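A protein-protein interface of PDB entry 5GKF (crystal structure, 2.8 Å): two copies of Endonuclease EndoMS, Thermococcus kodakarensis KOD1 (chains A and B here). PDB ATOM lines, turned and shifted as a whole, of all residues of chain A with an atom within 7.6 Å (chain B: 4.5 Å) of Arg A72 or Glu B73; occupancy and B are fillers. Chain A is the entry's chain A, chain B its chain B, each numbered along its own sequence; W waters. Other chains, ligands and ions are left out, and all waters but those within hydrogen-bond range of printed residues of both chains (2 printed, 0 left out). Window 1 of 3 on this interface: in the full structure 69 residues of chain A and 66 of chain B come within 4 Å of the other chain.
NZ of Lys A59 lies within hydrogen-bond range of O of Lys B71 (3.0 Å). The side-chain hydroxyl of Ser A63 sits at hydrogen-bond distance from the backbone carbonyl oxygen of Lys B71, 2.8 Å away. NH2 of Arg A72 is in salt-bridge range of OE1 of Glu B73. NZ of Lys A59 lies within hydrogen-bond range of O of Lys B70 (2.7 Å). OE1 of Glu A73 is in salt-bridge range of NH2 of Arg B72 (3.6 Å). O of Lys A71 sits at hydrogen-bond distance from OG of Ser B63. The side-chain amino group (NZ) of Lys A59 is in hydrogen-bond range of a ring nitrogen (ND1) of His B67, 3.0 Å away.
The guanidinium group (NH1) of Arg B72 lies within salt-bridge range of the side-chain carboxylate (OE2) of Glu B73 (2.4 Å). NE of Arg A72 lies within salt-bridge range of OE2 of Glu A73 (2.8 Å).
CD1 of Leu A65 touches CE1 of His B67, 3.5 Å away. Arg B72 touches Leu A65 (CG to CD2, 3.8 Å). His A67 touches Leu B65. Pro B80 touches Lys A71. CG of Arg A72 touches CD2 of Leu B65, at 3.6 Å. Arg A72 touches Pro B74. Arg B72 touches Pro A74 (NH2 to CD, 3.7 Å). Trp A77 touches Arg B72 (CD1 to NE, 3.2 Å). Lys B71 touches Pro A80 (CA to CG, 3.98 Å). Arg B72 touches Pro A80.
Of the printed residues of chain B, Arg A72 touches Leu B65 (3.6 Å), Glu B73 (2.7 Å), Pro B74 (3.5 Å) and Trp B77 (3.2 Å). Printed residues of chain B within 4 Å of Pro A80: Lys B71 (3.98 Å) and Arg B72 (3.9 Å). Printed residues of chain A within 4 Å of Arg B72: Ser A63 (3.9 Å), Leu A65 (3.8 Å), Glu A73 (3.6 Å), Pro A74 (3.7 Å), Trp A77 (3.2 Å) and Pro A80 (3.9 Å). Printed residues of chain A within 4 Å of Pro B80: Lys A71. Printed residues of chain A within 4 Å of Lys B71: Lys A59 (3.0 Å), Ser A63 (2.8 Å) and Pro A80 (3.98 Å). Of the printed residues of chain A, Leu B65 touches His A67 and Arg A72. Val B75 touches none of the printed residues of chain A.
Hydrophobic or aromatic side chains of chain A that line the printed part of chain B: Leu A65, His A67, Pro A74, Trp A77 and Pro A80. Among the printed residues, 19 pairs touch across the chains.
Ser A63 touches Lys B71, and with the chains exchanged Lys A71 touches Ser B63. Ser A63 touches Arg B72, but with the chains exchanged Arg A72 does not touch Ser B63 (4.01 Å). Leu A65 touches His B67, and with the chains exchanged His A67 touches Leu B65. Arg A72 touches Glu B73, and with the chains exchanged Glu A73 touches Arg B72. Positions printed for both chains: 63, 65, 67, 70, 71, 72, 73, 74, 75, 77 and 80. Of the 19 pairs that touch across the chains among the printed residues, 14 have their exchanged pair printed and touching as well.
Water W1 lies within hydrogen-bond range of NE2 of His B67 (2.8 Å) and NE2 of His A67 (3.0 Å). Water W2 lies within hydrogen-bond range of the backbone carbonyl oxygen of Glu B73 (2.9 Å), the backbone carbonyl oxygen of Lys B70 (3.0 Å), the side-chain amino group of Lys A59 (3.2 Å) and the backbone NH of Val B75 (3.5 Å).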
ATOM      1  N   LYS A  59     -27.154 -24.835  25.682  1.00  0.00           N
ATOM      2  CA  LYS A  59     -28.547 -24.392  25.657  1.00  0.00           C
ATOM      3  C   LYS A  59     -29.404 -25.168  26.648  1.00  0.00           C
ATOM      4  O   LYS A  59     -29.114 -26.325  26.946  1.00  0.00           O
ATOM      5  CB  LYS A  59     -29.109 -24.511  24.250  1.00  0.00           C
ATOM      6  CG  LYS A  59     -28.338 -23.715  23.222  1.00  0.00           C
ATOM      7  CD  LYS A  59     -28.936 -23.962  21.860  1.00  0.00           C
ATOM      8  CE  LYS A  59     -28.608 -22.865  20.888  1.00  0.00           C
ATOM      9  NZ  LYS A  59     -29.332 -23.136  19.642  1.00  0.00           N
ATOM     10  N   SER A  63     -28.316 -28.766  24.232  1.00  0.00           N
ATOM     11  CA  SER A  63     -27.369 -28.528  23.129  1.00  0.00           C
ATOM     12  C   SER A  63     -26.075 -27.928  23.659  1.00  0.00           C
ATOM     13  O   SER A  63     -26.068 -27.098  24.572  1.00  0.00           O
ATOM     14  CB  SER A  63     -27.956 -27.630  22.062  1.00  0.00           C
ATOM     15  OG  SER A  63     -29.232 -28.096  21.691  1.00  0.00           O
ATOM     16  N   LEU A  65     -22.277 -26.609  22.258  1.00  0.00           N
ATOM     17  CA  LEU A  65     -21.554 -26.243  21.025  1.00  0.00           C
ATOM     18  C   LEU A  65     -20.178 -25.689  21.329  1.00  0.00           C
ATOM     19  O   LEU A  65     -20.015 -24.829  22.194  1.00  0.00           O
ATOM     20  CB  LEU A  65     -22.332 -25.225  20.201  1.00  0.00           C
ATOM     21  CG  LEU A  65     -23.863 -25.300  20.262  1.00  0.00           C
ATOM     22  CD1 LEU A  65     -24.529 -24.176  19.460  1.00  0.00           C
ATOM     23  CD2 LEU A  65     -24.330 -26.627  19.750  1.00  0.00           C
ATOM     24  N   HIS A  67     -17.369 -23.669  19.380  1.00  0.00           N
ATOM     25  CA  HIS A  67     -17.069 -22.928  18.157  1.00  0.00           C
ATOM     26  C   HIS A  67     -15.639 -22.399  18.085  1.00  0.00           C
ATOM     27  O   HIS A  67     -15.130 -21.816  19.031  1.00  0.00           O
ATOM     28  CB  HIS A  67     -18.029 -21.767  17.997  1.00  0.00           C
ATOM     29  CG  HIS A  67     -19.331 -22.143  17.357  1.00  0.00           C
ATOM     30  ND1 HIS A  67     -19.495 -22.210  15.993  1.00  0.00           N
ATOM     31  CD2 HIS A  67     -20.538 -22.436  17.897  1.00  0.00           C
ATOM     32  CE1 HIS A  67     -20.741 -22.551  15.717  1.00  0.00           C
ATOM     33  NE2 HIS A  67     -21.393 -22.694  16.853  1.00  0.00           N
ATOM     34  N   LYS A  70     -13.641 -20.081  12.868  1.00  0.00           N
ATOM     35  CA  LYS A  70     -14.034 -20.279  11.494  1.00  0.00           C
ATOM     36  C   LYS A  70     -15.163 -21.285  11.336  1.00  0.00           C
ATOM     37  O   LYS A  70     -15.518 -22.026  12.254  1.00  0.00           O
ATOM     38  CB  LYS A  70     -12.813 -20.681  10.664  1.00  0.00           C
ATOM     39  CG  LYS A  70     -11.936 -19.465  10.318  1.00  0.00           C
ATOM     40  CD  LYS A  70     -10.638 -19.826   9.623  1.00  0.00           C
ATOM     41  CE  LYS A  70      -9.603 -18.760   9.918  1.00  0.00           C
ATOM     42  NZ  LYS A  70      -8.341 -19.073   9.203  1.00  0.00           N
ATOM     43  N   LYS A  71     -15.690 -21.251  10.120  1.00  0.00           N
ATOM     44  CA  LYS A  71     -16.851 -21.961   9.544  1.00  0.00           C
ATOM     45  C   LYS A  71     -18.264 -21.813  10.173  1.00  0.00           C
ATOM     46  O   LYS A  71     -18.460 -21.023  11.091  1.00  0.00           O
ATOM     47  CB  LYS A  71     -16.424 -23.425   9.520  1.00  0.00           C
ATOM     48  CG  LYS A  71     -14.974 -23.576   8.915  1.00  0.00           C
ATOM     49  CD  LYS A  71     -14.565 -25.019   8.649  1.00  0.00           C
ATOM     50  CE  LYS A  71     -13.073 -25.158   8.286  1.00  0.00           C
ATOM     51  NZ  LYS A  71     -12.648 -26.619   8.226  1.00  0.00           N
ATOM     52  N   ARG A  72     -19.245 -22.610   9.762  1.00  0.00           N
ATOM     53  CA  ARG A  72     -20.589 -22.381  10.323  1.00  0.00           C
ATOM     54  C   ARG A  72     -20.916 -23.399  11.404  1.00  0.00           C
ATOM     55  O   ARG A  72     -21.804 -23.201  12.260  1.00  0.00           O
ATOM     56  CB  ARG A  72     -21.672 -22.407   9.246  1.00  0.00           C
ATOM     57  CG  ARG A  72     -22.977 -21.846   9.782  1.00  0.00           C
ATOM     58  CD  ARG A  72     -24.232 -22.454   9.189  1.00  0.00           C
ATOM     59  NE  ARG A  72     -24.448 -23.880   9.439  1.00  0.00           N
ATOM     60  CZ  ARG A  72     -25.645 -24.452   9.627  1.00  0.00           C
ATOM     61  NH1 ARG A  72     -26.767 -23.740   9.642  1.00  0.00           N
ATOM     62  NH2 ARG A  72     -25.723 -25.755   9.845  1.00  0.00           N
ATOM     63  N   GLU A  73     -20.136 -24.467  11.360  1.00  0.00           N
ATOM     64  CA  GLU A  73     -20.303 -25.624  12.191  1.00  0.00           C
ATOM     65  C   GLU A  73     -19.437 -25.537  13.423  1.00  0.00           C
ATOM     66  O   GLU A  73     -18.298 -25.100  13.361  1.00  0.00           O
ATOM     67  CB  GLU A  73     -19.963 -26.862  11.400  1.00  0.00           C
ATOM     68  CG  GLU A  73     -20.739 -26.967  10.149  1.00  0.00           C
ATOM     69  CD  GLU A  73     -22.192 -27.015  10.436  1.00  0.00           C
ATOM     70  OE1 GLU A  73     -22.609 -27.957  11.144  1.00  0.00           O
ATOM     71  OE2 GLU A  73     -22.914 -26.111   9.959  1.00  0.00           O
ATOM     72  N   PRO A  74     -19.973 -25.968  14.558  1.00  0.00           N
ATOM     73  CA  PRO A  74     -19.086 -26.013  15.709  1.00  0.00           C
ATOM     74  C   PRO A  74     -18.082 -27.141  15.489  1.00  0.00           C
ATOM     75  O   PRO A  74     -18.421 -28.128  14.829  1.00  0.00           O
ATOM     76  CB  PRO A  74     -20.044 -26.286  16.856  1.00  0.00           C
ATOM     77  CG  PRO A  74     -21.114 -27.128  16.204  1.00  0.00           C
ATOM     78  CD  PRO A  74     -21.274 -26.608  14.818  1.00  0.00           C
ATOM     79  N   VAL A  75     -16.855 -26.997  15.981  1.00  0.00           N
ATOM     80  CA  VAL A  75     -15.879 -28.069  15.759  1.00  0.00           C
ATOM     81  C   VAL A  75     -16.300 -29.352  16.480  1.00  0.00           C
ATOM     82  O   VAL A  75     -16.188 -30.461  15.940  1.00  0.00           O
ATOM     83  CB  VAL A  75     -14.489 -27.673  16.210  1.00  0.00           C
ATOM     84  CG1 VAL A  75     -14.545 -26.949  17.544  1.00  0.00           C
ATOM     85  CG2 VAL A  75     -13.633 -28.896  16.314  1.00  0.00           C
ATOM     86  N   TRP A  77     -19.607 -30.750  19.338  1.00  0.00           N
ATOM     87  CA  TRP A  77     -20.980 -30.436  19.709  1.00  0.00           C
ATOM     88  C   TRP A  77     -21.668 -31.653  20.222  1.00  0.00           C
ATOM     89  O   TRP A  77     -21.228 -32.753  20.002  1.00  0.00           O
ATOM     90  CB  TRP A  77     -21.805 -29.897  18.521  1.00  0.00           C
ATOM     91  CG  TRP A  77     -22.184 -31.001  17.551  1.00  0.00           C
ATOM     92  CD1 TRP A  77     -23.365 -31.699  17.502  1.00  0.00           C
ATOM     93  CD2 TRP A  77     -21.349 -31.555  16.528  1.00  0.00           C
ATOM     94  NE1 TRP A  77     -23.314 -32.645  16.509  1.00  0.00           N
ATOM     95  CE2 TRP A  77     -22.099 -32.578  15.894  1.00  0.00           C
ATOM     96  CE3 TRP A  77     -20.054 -31.285  16.083  1.00  0.00           C
ATOM     97  CZ2 TRP A  77     -21.583 -33.326  14.836  1.00  0.00           C
ATOM     98  CZ3 TRP A  77     -19.550 -32.024  15.037  1.00  0.00           C
ATOM     99  CH2 TRP A  77     -20.314 -33.035  14.418  1.00  0.00           C
ATOM    100  N   PRO A  80     -29.467 -31.707  21.189  1.00  0.00           N
ATOM    101  CA  PRO A  80     -30.372 -31.645  22.350  1.00  0.00           C
ATOM    102  C   PRO A  80     -30.541 -32.961  23.111  1.00  0.00           C
ATOM    103  O   PRO A  80     -30.416 -34.032  22.560  1.00  0.00           O
ATOM    104  CB  PRO A  80     -31.705 -31.259  21.730  1.00  0.00           C
ATOM    105  CG  PRO A  80     -31.344 -30.492  20.526  1.00  0.00           C
ATOM    106  CD  PRO A  80     -30.037 -31.019  20.017  1.00  0.00           C
ATOM    107  N   SER B  63     -18.941 -15.963   8.710  1.00  0.00           N
ATOM    108  CA  SER B  63     -20.023 -16.763   9.261  1.00  0.00           C
ATOM    109  C   SER B  63     -20.848 -15.951  10.232  1.00  0.00           C
ATOM    110  O   SER B  63     -20.318 -15.245  11.077  1.00  0.00           O
ATOM    111  CB  SER B  63     -19.466 -17.996   9.950  1.00  0.00           C
ATOM    112  OG  SER B  63     -18.641 -18.707   9.052  1.00  0.00           O
ATOM    113  N   LEU B  65     -24.263 -16.183  12.720  1.00  0.00           N
ATOM    114  CA  LEU B  65     -25.167 -17.119  13.379  1.00  0.00           C
ATOM    115  C   LEU B  65     -26.193 -16.422  14.265  1.00  0.00           C
ATOM    116  O   LEU B  65     -25.854 -15.509  15.015  1.00  0.00           O
ATOM    117  CB  LEU B  65     -24.365 -18.108  14.224  1.00  0.00           C
ATOM    118  CG  LEU B  65     -23.218 -18.769  13.477  1.00  0.00           C
ATOM    119  CD1 LEU B  65     -22.491 -19.759  14.348  1.00  0.00           C
ATOM    120  CD2 LEU B  65     -23.788 -19.428  12.273  1.00  0.00           C
ATOM    121  N   HIS B  67     -28.687 -17.874  17.145  1.00  0.00           N
ATOM    122  CA  HIS B  67     -29.137 -19.037  17.921  1.00  0.00           C
ATOM    123  C   HIS B  67     -30.293 -18.739  18.905  1.00  0.00           C
ATOM    124  O   HIS B  67     -30.177 -17.866  19.756  1.00  0.00           O
ATOM    125  CB  HIS B  67     -27.960 -19.617  18.707  1.00  0.00           C
ATOM    126  CG  HIS B  67     -27.091 -20.561  17.922  1.00  0.00           C
ATOM    127  ND1 HIS B  67     -27.411 -21.892  17.738  1.00  0.00           N
ATOM    128  CD2 HIS B  67     -25.893 -20.379  17.314  1.00  0.00           C
ATOM    129  CE1 HIS B  67     -26.463 -22.478  17.028  1.00  0.00           C
ATOM    130  NE2 HIS B  67     -25.530 -21.584  16.757  1.00  0.00           N
ATOM    131  N   LYS B  70     -33.039 -22.851  21.958  1.00  0.00           N
ATOM    132  CA  LYS B  70     -33.128 -24.271  21.664  1.00  0.00           C
ATOM    133  C   LYS B  70     -32.452 -24.691  20.375  1.00  0.00           C
ATOM    134  O   LYS B  70     -31.936 -23.902  19.597  1.00  0.00           O
ATOM    135  CB  LYS B  70     -34.577 -24.707  21.604  1.00  0.00           C
ATOM    136  CG  LYS B  70     -35.273 -24.764  22.942  1.00  0.00           C
ATOM    137  CD  LYS B  70     -36.788 -24.906  22.754  1.00  0.00           C
ATOM    138  CE  LYS B  70     -37.525 -24.936  24.092  1.00  0.00           C
ATOM    139  NZ  LYS B  70     -37.089 -23.836  25.012  1.00  0.00           N
ATOM    140  N   LYS B  71     -32.524 -25.988  20.187  1.00  0.00           N
ATOM    141  CA  LYS B  71     -31.904 -26.802  19.155  1.00  0.00           C
ATOM    142  C   LYS B  71     -30.383 -26.720  19.018  1.00  0.00           C
ATOM    143  O   LYS B  71     -29.721 -26.069  19.823  1.00  0.00           O
ATOM    144  CB  LYS B  71     -32.567 -26.409  17.838  1.00  0.00           C
ATOM    145  CG  LYS B  71     -34.081 -26.417  17.951  1.00  0.00           C
ATOM    146  CD  LYS B  71     -34.775 -26.766  16.655  1.00  0.00           C
ATOM    147  CE  LYS B  71     -36.195 -27.202  16.944  1.00  0.00           C
ATOM    148  NZ  LYS B  71     -36.216 -28.325  17.944  1.00  0.00           N
ATOM    149  N   ARG B  72     -29.832 -27.309  17.957  1.00  0.00           N
ATOM    150  CA  ARG B  72     -28.375 -27.330  17.812  1.00  0.00           C
ATOM    151  C   ARG B  72     -27.977 -26.449  16.635  1.00  0.00           C
ATOM    152  O   ARG B  72     -26.824 -26.044  16.448  1.00  0.00           O
ATOM    153  CB  ARG B  72     -27.891 -28.784  17.657  1.00  0.00           C
ATOM    154  CG  ARG B  72     -26.374 -28.982  17.569  1.00  0.00           C
ATOM    155  CD  ARG B  72     -26.009 -28.965  16.124  1.00  0.00           C
ATOM    156  NE  ARG B  72     -24.642 -29.292  15.792  1.00  0.00           N
ATOM    157  CZ  ARG B  72     -24.282 -29.517  14.535  1.00  0.00           C
ATOM    158  NH1 ARG B  72     -25.217 -29.441  13.609  1.00  0.00           N
ATOM    159  NH2 ARG B  72     -23.028 -29.817  14.198  1.00  0.00           N
ATOM    160  N   GLU B  73     -28.998 -26.136  15.864  1.00  0.00           N
ATOM    161  CA  GLU B  73     -28.877 -25.347  14.680  1.00  0.00           C
ATOM    162  C   GLU B  73     -29.227 -23.882  14.955  1.00  0.00           C
ATOM    163  O   GLU B  73     -30.184 -23.568  15.680  1.00  0.00           O
ATOM    164  CB  GLU B  73     -29.778 -25.941  13.595  1.00  0.00           C
ATOM    165  CG  GLU B  73     -29.325 -27.286  13.121  1.00  0.00           C
ATOM    166  CD  GLU B  73     -27.921 -27.229  12.534  1.00  0.00           C
ATOM    167  OE1 GLU B  73     -27.698 -26.455  11.566  1.00  0.00           O
ATOM    168  OE2 GLU B  73     -27.037 -27.934  13.060  1.00  0.00           O
ATOM    169  N   PRO B  74     -28.430 -22.973  14.414  1.00  0.00           N
ATOM    170  CA  PRO B  74     -28.913 -21.587  14.383  1.00  0.00           C
ATOM    171  C   PRO B  74     -30.305 -21.486  13.721  1.00  0.00           C
ATOM    172  O   PRO B  74     -30.558 -22.180  12.718  1.00  0.00           O
ATOM    173  CB  PRO B  74     -27.855 -20.881  13.533  1.00  0.00           C
ATOM    174  CG  PRO B  74     -27.257 -22.035  12.668  1.00  0.00           C
ATOM    175  CD  PRO B  74     -27.179 -23.153  13.658  1.00  0.00           C
ATOM    176  N   VAL B  75     -31.194 -20.658  14.277  1.00  0.00           N
ATOM    177  CA  VAL B  75     -32.475 -20.385  13.627  1.00  0.00           C
ATOM    178  C   VAL B  75     -32.287 -19.677  12.238  1.00  0.00           C
ATOM    179  O   VAL B  75     -32.971 -20.006  11.268  1.00  0.00           O
ATOM    180  CB  VAL B  75     -33.396 -19.565  14.568  1.00  0.00           C
ATOM    181  CG1 VAL B  75     -32.793 -18.178  14.898  1.00  0.00           C
ATOM    182  CG2 VAL B  75     -34.828 -19.486  13.986  1.00  0.00           C
ATOM    183  N   TRP B  77     -28.828 -18.086   9.636  1.00  0.00           N
ATOM    184  CA  TRP B  77     -27.384 -17.979   9.475  1.00  0.00           C
ATOM    185  C   TRP B  77     -26.985 -17.491   8.118  1.00  0.00           C
ATOM    186  O   TRP B  77     -27.787 -17.509   7.178  1.00  0.00           O
ATOM    187  CB  TRP B  77     -26.700 -19.333   9.689  1.00  0.00           C
ATOM    188  CG  TRP B  77     -27.005 -20.272   8.595  1.00  0.00           C
ATOM    189  CD1 TRP B  77     -26.212 -20.582   7.542  1.00  0.00           C
ATOM    190  CD2 TRP B  77     -28.220 -20.993   8.405  1.00  0.00           C
ATOM    191  NE1 TRP B  77     -26.827 -21.480   6.728  1.00  0.00           N
ATOM    192  CE2 TRP B  77     -28.075 -21.753   7.231  1.00  0.00           C
ATOM    193  CE3 TRP B  77     -29.421 -21.086   9.127  1.00  0.00           C
ATOM    194  CZ2 TRP B  77     -29.075 -22.603   6.756  1.00  0.00           C
ATOM    195  CZ3 TRP B  77     -30.400 -21.911   8.660  1.00  0.00           C
ATOM    196  CH2 TRP B  77     -30.227 -22.667   7.479  1.00  0.00           C
ATOM    197  N   PRO B  80     -19.695 -19.108   5.718  1.00  0.00           N
ATOM    198  CA  PRO B  80     -18.447 -18.338   5.590  1.00  0.00           C
ATOM    199  C   PRO B  80     -18.319 -17.626   4.230  1.00  0.00           C
ATOM    200  O   PRO B  80     -18.674 -18.205   3.214  1.00  0.00           O
ATOM    201  CB  PRO B  80     -17.354 -19.399   5.760  1.00  0.00           C
ATOM    202  CG  PRO B  80     -17.976 -20.517   6.491  1.00  0.00           C
ATOM    203  CD  PRO B  80     -19.463 -20.492   6.164  1.00  0.00           C
HETATM  204  O   HOH W   1     -23.873 -23.195  15.209  1.00  0.00           O
HETATM  205  O   HOH W   2     -31.411 -21.765  17.576  1.00  0.00           O
